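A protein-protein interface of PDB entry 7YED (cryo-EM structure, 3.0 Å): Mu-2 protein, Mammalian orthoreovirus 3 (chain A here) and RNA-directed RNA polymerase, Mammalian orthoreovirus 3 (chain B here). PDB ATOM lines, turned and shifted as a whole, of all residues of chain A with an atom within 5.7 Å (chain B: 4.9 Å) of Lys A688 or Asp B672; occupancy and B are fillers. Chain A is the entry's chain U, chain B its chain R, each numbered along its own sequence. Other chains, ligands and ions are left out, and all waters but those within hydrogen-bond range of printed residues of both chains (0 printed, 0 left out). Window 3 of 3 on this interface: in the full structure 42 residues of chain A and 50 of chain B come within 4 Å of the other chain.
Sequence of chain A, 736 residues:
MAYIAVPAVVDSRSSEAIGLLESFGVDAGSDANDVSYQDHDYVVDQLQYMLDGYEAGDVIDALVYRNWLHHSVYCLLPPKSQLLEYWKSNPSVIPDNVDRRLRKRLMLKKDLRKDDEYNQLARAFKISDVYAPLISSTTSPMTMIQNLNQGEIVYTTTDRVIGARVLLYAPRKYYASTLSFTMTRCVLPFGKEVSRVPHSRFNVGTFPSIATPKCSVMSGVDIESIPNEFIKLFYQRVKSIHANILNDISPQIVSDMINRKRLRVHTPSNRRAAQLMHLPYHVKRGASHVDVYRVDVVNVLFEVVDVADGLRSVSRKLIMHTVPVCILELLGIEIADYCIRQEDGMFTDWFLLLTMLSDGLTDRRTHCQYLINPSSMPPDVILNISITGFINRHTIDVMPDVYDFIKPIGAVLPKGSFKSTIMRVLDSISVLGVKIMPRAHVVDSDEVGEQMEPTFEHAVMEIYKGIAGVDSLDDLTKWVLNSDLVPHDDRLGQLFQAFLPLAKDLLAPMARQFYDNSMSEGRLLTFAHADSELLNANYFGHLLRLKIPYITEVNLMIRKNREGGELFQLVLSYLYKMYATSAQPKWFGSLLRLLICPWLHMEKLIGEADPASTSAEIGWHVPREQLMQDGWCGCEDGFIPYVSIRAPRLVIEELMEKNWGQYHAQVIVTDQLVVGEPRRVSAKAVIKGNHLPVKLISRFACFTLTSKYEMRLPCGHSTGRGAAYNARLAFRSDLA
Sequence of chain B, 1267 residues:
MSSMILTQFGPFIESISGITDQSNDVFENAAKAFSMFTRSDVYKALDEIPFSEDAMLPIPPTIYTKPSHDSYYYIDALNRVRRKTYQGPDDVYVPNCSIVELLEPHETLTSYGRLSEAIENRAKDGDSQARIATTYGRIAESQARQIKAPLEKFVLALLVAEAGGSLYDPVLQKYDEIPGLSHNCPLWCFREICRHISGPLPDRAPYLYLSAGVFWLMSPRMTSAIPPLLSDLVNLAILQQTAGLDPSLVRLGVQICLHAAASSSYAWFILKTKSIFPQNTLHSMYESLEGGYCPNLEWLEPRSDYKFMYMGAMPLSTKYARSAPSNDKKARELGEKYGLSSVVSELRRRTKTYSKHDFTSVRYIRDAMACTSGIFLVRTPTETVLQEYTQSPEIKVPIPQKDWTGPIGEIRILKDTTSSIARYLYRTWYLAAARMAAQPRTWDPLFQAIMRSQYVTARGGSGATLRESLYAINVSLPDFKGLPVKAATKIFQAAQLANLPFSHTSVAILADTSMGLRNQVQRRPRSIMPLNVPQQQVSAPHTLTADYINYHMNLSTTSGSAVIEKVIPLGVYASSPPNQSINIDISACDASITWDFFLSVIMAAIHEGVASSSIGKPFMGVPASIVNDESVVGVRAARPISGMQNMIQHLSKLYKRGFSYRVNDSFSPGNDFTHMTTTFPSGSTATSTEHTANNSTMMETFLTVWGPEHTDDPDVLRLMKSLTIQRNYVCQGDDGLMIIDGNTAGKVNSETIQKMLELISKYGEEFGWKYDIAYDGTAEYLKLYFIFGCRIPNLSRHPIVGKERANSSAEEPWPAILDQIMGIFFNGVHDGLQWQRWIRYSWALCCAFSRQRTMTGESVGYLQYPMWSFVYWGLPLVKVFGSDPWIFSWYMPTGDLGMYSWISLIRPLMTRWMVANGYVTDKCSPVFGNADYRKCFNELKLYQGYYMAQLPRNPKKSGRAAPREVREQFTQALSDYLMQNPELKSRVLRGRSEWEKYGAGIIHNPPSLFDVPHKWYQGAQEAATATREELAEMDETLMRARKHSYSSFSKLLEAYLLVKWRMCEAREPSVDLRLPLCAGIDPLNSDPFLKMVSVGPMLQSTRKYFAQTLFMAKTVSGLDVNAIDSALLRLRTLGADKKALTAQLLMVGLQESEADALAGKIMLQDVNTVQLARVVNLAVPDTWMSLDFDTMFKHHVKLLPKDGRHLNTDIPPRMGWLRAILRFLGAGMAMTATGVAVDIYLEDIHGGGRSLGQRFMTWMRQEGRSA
Of the printed residues of chain B, Gln A666 touches Asn B79 (3.5 Å).
Val A686 touches none of the printed residues of chain B.
Lys A688 touches just these residues of chain B: Gly B670 (3.4 Å) and Asp B672 (3.0 Å).
Of the printed residues of chain B, Gly A689 touches Asp B672.
Of the printed residues of chain A, Asn B79 touches Gln A666.
Of the printed residues of chain A, Gly B670 touches Lys A688 (3.4 Å).
Asp B672 touches just these residues of chain A: Lys A688 (3.0 Å) and Gly A689 (3.4 Å).
The nearest residue of chain A that does not touch Asp B672 is Ile A687 (5.0 Å).
The backbone carbonyl oxygen (O) of Gly B670 lies within hydrogen-bond range of the side-chain amino group (NZ) of Lys A688, at 3.4 Å.
The side-chain carboxylate of Asp B672 lies within salt-bridge range of the side-chain amino group of Lys A688 (3.8 Å).
The side-chain carboxylate (OD2) of Asp B672 is in hydrogen-bond range of the backbone NH (N) of Gly A689 (3.4 Å).
N of Gln A666 lies within hydrogen-bond range of O of Val A686 (3.2 Å).
O of His A664 is in hydrogen-bond range of N of Lys A688 (2.8 Å).
Printed residues of chain B that touch a printed residue of chain A: Asn B79, Gly B670 and Asp B672.
Along chain B the printed residues that touch a printed residue of chain A span positions 79 to 672.
Of the 9 printed residues of chain A, 3 touch a printed residue of chain B.
Printed residues of chain A that touch a printed residue of chain B: Gln A666, Lys A688 and Gly A689.
Among the printed residues, 4 pairs touch across the chains.
Among the printed residues, Asp or Glu carboxylates within 4 Å of a Lys or Arg side-chain nitrogen of the other chain: Lys A688 with Asp B672 (3.8 Å).
Gln A666 touches Asn B79 (CG to ND2, 3.5 Å).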
ATOM      1  N   TYR A 663     -15.053 -20.968  -3.007  1.00  0.00           N
ATOM      2  CA  TYR A 663     -15.058 -21.812  -1.821  1.00  0.00           C
ATOM      3  C   TYR A 663     -14.181 -23.025  -2.082  1.00  0.00           C
ATOM      4  O   TYR A 663     -14.417 -23.767  -3.040  1.00  0.00           O
ATOM      5  CB  TYR A 663     -16.485 -22.226  -1.459  1.00  0.00           C
ATOM      6  CG  TYR A 663     -17.327 -21.052  -1.028  1.00  0.00           C
ATOM      7  CD1 TYR A 663     -17.231 -20.546   0.256  1.00  0.00           C
ATOM      8  CD2 TYR A 663     -18.197 -20.435  -1.910  1.00  0.00           C
ATOM      9  CE1 TYR A 663     -17.987 -19.468   0.654  1.00  0.00           C
ATOM     10  CE2 TYR A 663     -18.959 -19.354  -1.519  1.00  0.00           C
ATOM     11  CZ  TYR A 663     -18.849 -18.877  -0.234  1.00  0.00           C
ATOM     12  OH  TYR A 663     -19.601 -17.801   0.169  1.00  0.00           O
ATOM     13  N   HIS A 664     -13.172 -23.220  -1.239  1.00  0.00           N
ATOM     14  CA  HIS A 664     -12.149 -24.226  -1.460  1.00  0.00           C
ATOM     15  C   HIS A 664     -12.112 -25.208  -0.300  1.00  0.00           C
ATOM     16  O   HIS A 664     -12.548 -24.908   0.813  1.00  0.00           O
ATOM     17  CB  HIS A 664     -10.775 -23.573  -1.634  1.00  0.00           C
ATOM     18  CG  HIS A 664     -10.680 -22.674  -2.826  1.00  0.00           C
ATOM     19  ND1 HIS A 664     -10.580 -23.152  -4.114  1.00  0.00           N
ATOM     20  CD2 HIS A 664     -10.680 -21.324  -2.926  1.00  0.00           C
ATOM     21  CE1 HIS A 664     -10.518 -22.135  -4.956  1.00  0.00           C
ATOM     22  NE2 HIS A 664     -10.578 -21.015  -4.260  1.00  0.00           N
ATOM     23  N   ALA A 665     -11.568 -26.389  -0.571  1.00  0.00           N
ATOM     24  CA  ALA A 665     -11.436 -27.416   0.450  1.00  0.00           C
ATOM     25  C   ALA A 665     -10.547 -28.521  -0.090  1.00  0.00           C
ATOM     26  O   ALA A 665     -10.522 -28.773  -1.295  1.00  0.00           O
ATOM     27  CB  ALA A 665     -12.798 -27.983   0.858  1.00  0.00           C
ATOM     28  N   GLN A 666      -9.822 -29.173   0.812  1.00  0.00           N
ATOM     29  CA  GLN A 666      -8.912 -30.251   0.443  1.00  0.00           C
ATOM     30  C   GLN A 666      -9.683 -31.565   0.462  1.00  0.00           C
ATOM     31  O   GLN A 666     -10.025 -32.072   1.534  1.00  0.00           O
ATOM     32  CB  GLN A 666      -7.724 -30.309   1.395  1.00  0.00           C
ATOM     33  CG  GLN A 666      -6.819 -29.091   1.366  1.00  0.00           C
ATOM     34  CD  GLN A 666      -6.147 -28.886   0.026  1.00  0.00           C
ATOM     35  OE1 GLN A 666      -6.462 -27.944  -0.699  1.00  0.00           O
ATOM     36  NE2 GLN A 666      -5.212 -29.768  -0.311  1.00  0.00           N
ATOM     37  N   VAL A 686     -12.374 -30.935   3.680  1.00  0.00           N
ATOM     38  CA  VAL A 686     -12.166 -30.004   4.778  1.00  0.00           C
ATOM     39  C   VAL A 686     -12.201 -28.602   4.193  1.00  0.00           C
ATOM     40  O   VAL A 686     -11.271 -28.199   3.487  1.00  0.00           O
ATOM     41  CB  VAL A 686     -10.841 -30.248   5.510  1.00  0.00           C
ATOM     42  CG1 VAL A 686     -10.622 -29.185   6.561  1.00  0.00           C
ATOM     43  CG2 VAL A 686     -10.836 -31.628   6.133  1.00  0.00           C
ATOM     44  N   ILE A 687     -13.271 -27.857   4.480  1.00  0.00           N
ATOM     45  CA  ILE A 687     -13.425 -26.526   3.911  1.00  0.00           C
ATOM     46  C   ILE A 687     -12.322 -25.617   4.429  1.00  0.00           C
ATOM     47  O   ILE A 687     -11.885 -25.728   5.581  1.00  0.00           O
ATOM     48  CB  ILE A 687     -14.816 -25.962   4.243  1.00  0.00           C
ATOM     49  CG1 ILE A 687     -15.906 -26.832   3.622  1.00  0.00           C
ATOM     50  CG2 ILE A 687     -14.948 -24.538   3.749  1.00  0.00           C
ATOM     51  CD1 ILE A 687     -16.384 -27.944   4.516  1.00  0.00           C
ATOM     52  N   LYS A 688     -11.858 -24.714   3.570  1.00  0.00           N
ATOM     53  CA  LYS A 688     -10.791 -23.784   3.906  1.00  0.00           C
ATOM     54  C   LYS A 688     -11.268 -22.357   3.685  1.00  0.00           C
ATOM     55  O   LYS A 688     -11.824 -22.040   2.630  1.00  0.00           O
ATOM     56  CB  LYS A 688      -9.541 -24.059   3.070  1.00  0.00           C
ATOM     57  CG  LYS A 688      -8.947 -25.442   3.279  1.00  0.00           C
ATOM     58  CD  LYS A 688      -8.374 -25.593   4.678  1.00  0.00           C
ATOM     59  CE  LYS A 688      -7.697 -26.942   4.858  1.00  0.00           C
ATOM     60  NZ  LYS A 688      -7.168 -27.116   6.237  1.00  0.00           N
ATOM     61  N   GLY A 689     -11.043 -21.502   4.678  1.00  0.00           N
ATOM     62  CA  GLY A 689     -11.359 -20.090   4.565  1.00  0.00           C
ATOM     63  C   GLY A 689     -12.736 -19.686   5.055  1.00  0.00           C
ATOM     64  O   GLY A 689     -12.856 -19.039   6.099  1.00  0.00           O
ATOM     65  N   ASN A 690     -13.782 -20.052   4.319  1.00  0.00           N
ATOM     66  CA  ASN A 690     -15.131 -19.622   4.650  1.00  0.00           C
ATOM     67  C   ASN A 690     -16.110 -20.745   4.348  1.00  0.00           C
ATOM     68  O   ASN A 690     -15.839 -21.633   3.535  1.00  0.00           O
ATOM     69  CB  ASN A 690     -15.525 -18.359   3.875  1.00  0.00           C
ATOM     70  CG  ASN A 690     -14.758 -17.134   4.328  1.00  0.00           C
ATOM     71  OD1 ASN A 690     -14.540 -16.927   5.519  1.00  0.00           O
ATOM     72  ND2 ASN A 690     -14.347 -16.311   3.373  1.00  0.00           N
ATOM     73  N   LEU B  78      -7.940 -33.496  10.422  1.00  0.00           N
ATOM     74  CA  LEU B  78      -8.408 -32.279   9.776  1.00  0.00           C
ATOM     75  C   LEU B  78      -7.321 -31.609   8.946  1.00  0.00           C
ATOM     76  O   LEU B  78      -7.360 -30.391   8.736  1.00  0.00           O
ATOM     77  CB  LEU B  78      -8.952 -31.299  10.814  1.00  0.00           C
ATOM     78  CG  LEU B  78     -10.237 -31.705  11.529  1.00  0.00           C
ATOM     79  CD1 LEU B  78     -10.561 -30.706  12.619  1.00  0.00           C
ATOM     80  CD2 LEU B  78     -11.373 -31.797  10.537  1.00  0.00           C
ATOM     81  N   ASN B  79      -6.339 -32.382   8.482  1.00  0.00           N
ATOM     82  CA  ASN B  79      -5.294 -31.880   7.594  1.00  0.00           C
ATOM     83  C   ASN B  79      -4.430 -30.831   8.291  1.00  0.00           C
ATOM     84  O   ASN B  79      -3.861 -29.943   7.651  1.00  0.00           O
ATOM     85  CB  ASN B  79      -5.902 -31.327   6.303  1.00  0.00           C
ATOM     86  CG  ASN B  79      -4.877 -31.127   5.213  1.00  0.00           C
ATOM     87  OD1 ASN B  79      -3.695 -31.402   5.403  1.00  0.00           O
ATOM     88  ND2 ASN B  79      -5.320 -30.629   4.070  1.00  0.00           N
ATOM     89  N   VAL B 663      -8.299 -19.529  13.316  1.00  0.00           N
ATOM     90  CA  VAL B 663      -6.848 -19.625  13.385  1.00  0.00           C
ATOM     91  C   VAL B 663      -6.295 -19.712  11.973  1.00  0.00           C
ATOM     92  O   VAL B 663      -6.798 -20.477  11.144  1.00  0.00           O
ATOM     93  CB  VAL B 663      -6.413 -20.839  14.218  1.00  0.00           C
ATOM     94  CG1 VAL B 663      -4.907 -20.981  14.180  1.00  0.00           C
ATOM     95  CG2 VAL B 663      -6.898 -20.697  15.644  1.00  0.00           C
ATOM     96  N   ASN B 664      -5.270 -18.914  11.691  1.00  0.00           N
ATOM     97  CA  ASN B 664      -4.564 -18.972  10.412  1.00  0.00           C
ATOM     98  C   ASN B 664      -3.122 -18.548  10.690  1.00  0.00           C
ATOM     99  O   ASN B 664      -2.805 -17.357  10.683  1.00  0.00           O
ATOM    100  CB  ASN B 664      -5.224 -18.082   9.372  1.00  0.00           C
ATOM    101  CG  ASN B 664      -4.643 -18.274   7.987  1.00  0.00           C
ATOM    102  OD1 ASN B 664      -3.718 -19.060   7.789  1.00  0.00           O
ATOM    103  ND2 ASN B 664      -5.190 -17.554   7.016  1.00  0.00           N
ATOM    104  N   GLY B 670      -1.066 -24.530   5.437  1.00  0.00           N
ATOM    105  CA  GLY B 670      -2.213 -25.407   5.382  1.00  0.00           C
ATOM    106  C   GLY B 670      -3.072 -25.434   6.626  1.00  0.00           C
ATOM    107  O   GLY B 670      -3.941 -26.304   6.734  1.00  0.00           O
ATOM    108  N   ASN B 671      -2.860 -24.517   7.563  1.00  0.00           N
ATOM    109  CA  ASN B 671      -3.630 -24.457   8.803  1.00  0.00           C
ATOM    110  C   ASN B 671      -4.395 -23.138   8.826  1.00  0.00           C
ATOM    111  O   ASN B 671      -3.825 -22.089   9.139  1.00  0.00           O
ATOM    112  CB  ASN B 671      -2.719 -24.584  10.019  1.00  0.00           C
ATOM    113  CG  ASN B 671      -2.022 -25.919  10.086  1.00  0.00           C
ATOM    114  OD1 ASN B 671      -0.802 -26.002   9.974  1.00  0.00           O
ATOM    115  ND2 ASN B 671      -2.794 -26.976  10.279  1.00  0.00           N
ATOM    116  N   ASP B 672      -5.679 -23.187   8.486  1.00  0.00           N
ATOM    117  CA  ASP B 672      -6.564 -22.039   8.651  1.00  0.00           C
ATOM    118  C   ASP B 672      -7.908 -22.488   9.204  1.00  0.00           C
ATOM    119  O   ASP B 672      -8.964 -21.980   8.814  1.00  0.00           O
ATOM    120  CB  ASP B 672      -6.736 -21.269   7.342  1.00  0.00           C
ATOM    121  CG  ASP B 672      -7.367 -22.101   6.243  1.00  0.00           C
ATOM    122  OD1 ASP B 672      -7.608 -23.307   6.451  1.00  0.00           O
ATOM    123  OD2 ASP B 672      -7.628 -21.540   5.159  1.00  0.00           O
ATOM    124  N   PHE B 673      -7.883 -23.449  10.120  1.00  0.00           N
ATOM    125  CA  PHE B 673      -9.103 -24.011  10.668  1.00  0.00           C
ATOM    126  C   PHE B 673      -9.854 -22.972  11.497  1.00  0.00           C
ATOM    127  O   PHE B 673      -9.383 -21.854  11.730  1.00  0.00           O
ATOM    128  CB  PHE B 673      -8.781 -25.242  11.516  1.00  0.00           C
ATOM    129  CG  PHE B 673      -7.933 -24.945  12.720  1.00  0.00           C
ATOM    130  CD1 PHE B 673      -6.554 -24.916  12.623  1.00  0.00           C
ATOM    131  CD2 PHE B 673      -8.511 -24.719  13.955  1.00  0.00           C
ATOM    132  CE1 PHE B 673      -5.773 -24.649  13.725  1.00  0.00           C
ATOM    133  CE2 PHE B 673      -7.731 -24.453  15.061  1.00  0.00           C
ATOM    134  CZ  PHE B 673      -6.361 -24.419  14.945  1.00  0.00           C
ATOM    135  N   THR B 674     -11.045 -23.357  11.939  1.00  0.00           N
ATOM    136  CA  THR B 674     -11.836 -22.572  12.873  1.00  0.00           C
ATOM    137  C   THR B 674     -12.132 -23.425  14.097  1.00  0.00           C
ATOM    138  O   THR B 674     -12.452 -24.610  13.976  1.00  0.00           O
ATOM    139  CB  THR B 674     -13.137 -22.080  12.235  1.00  0.00           C
ATOM    140  OG1 THR B 674     -13.816 -21.201  13.139  1.00  0.00           O
ATOM    141  CG2 THR B 674     -14.037 -23.247  11.895  1.00  0.00           C
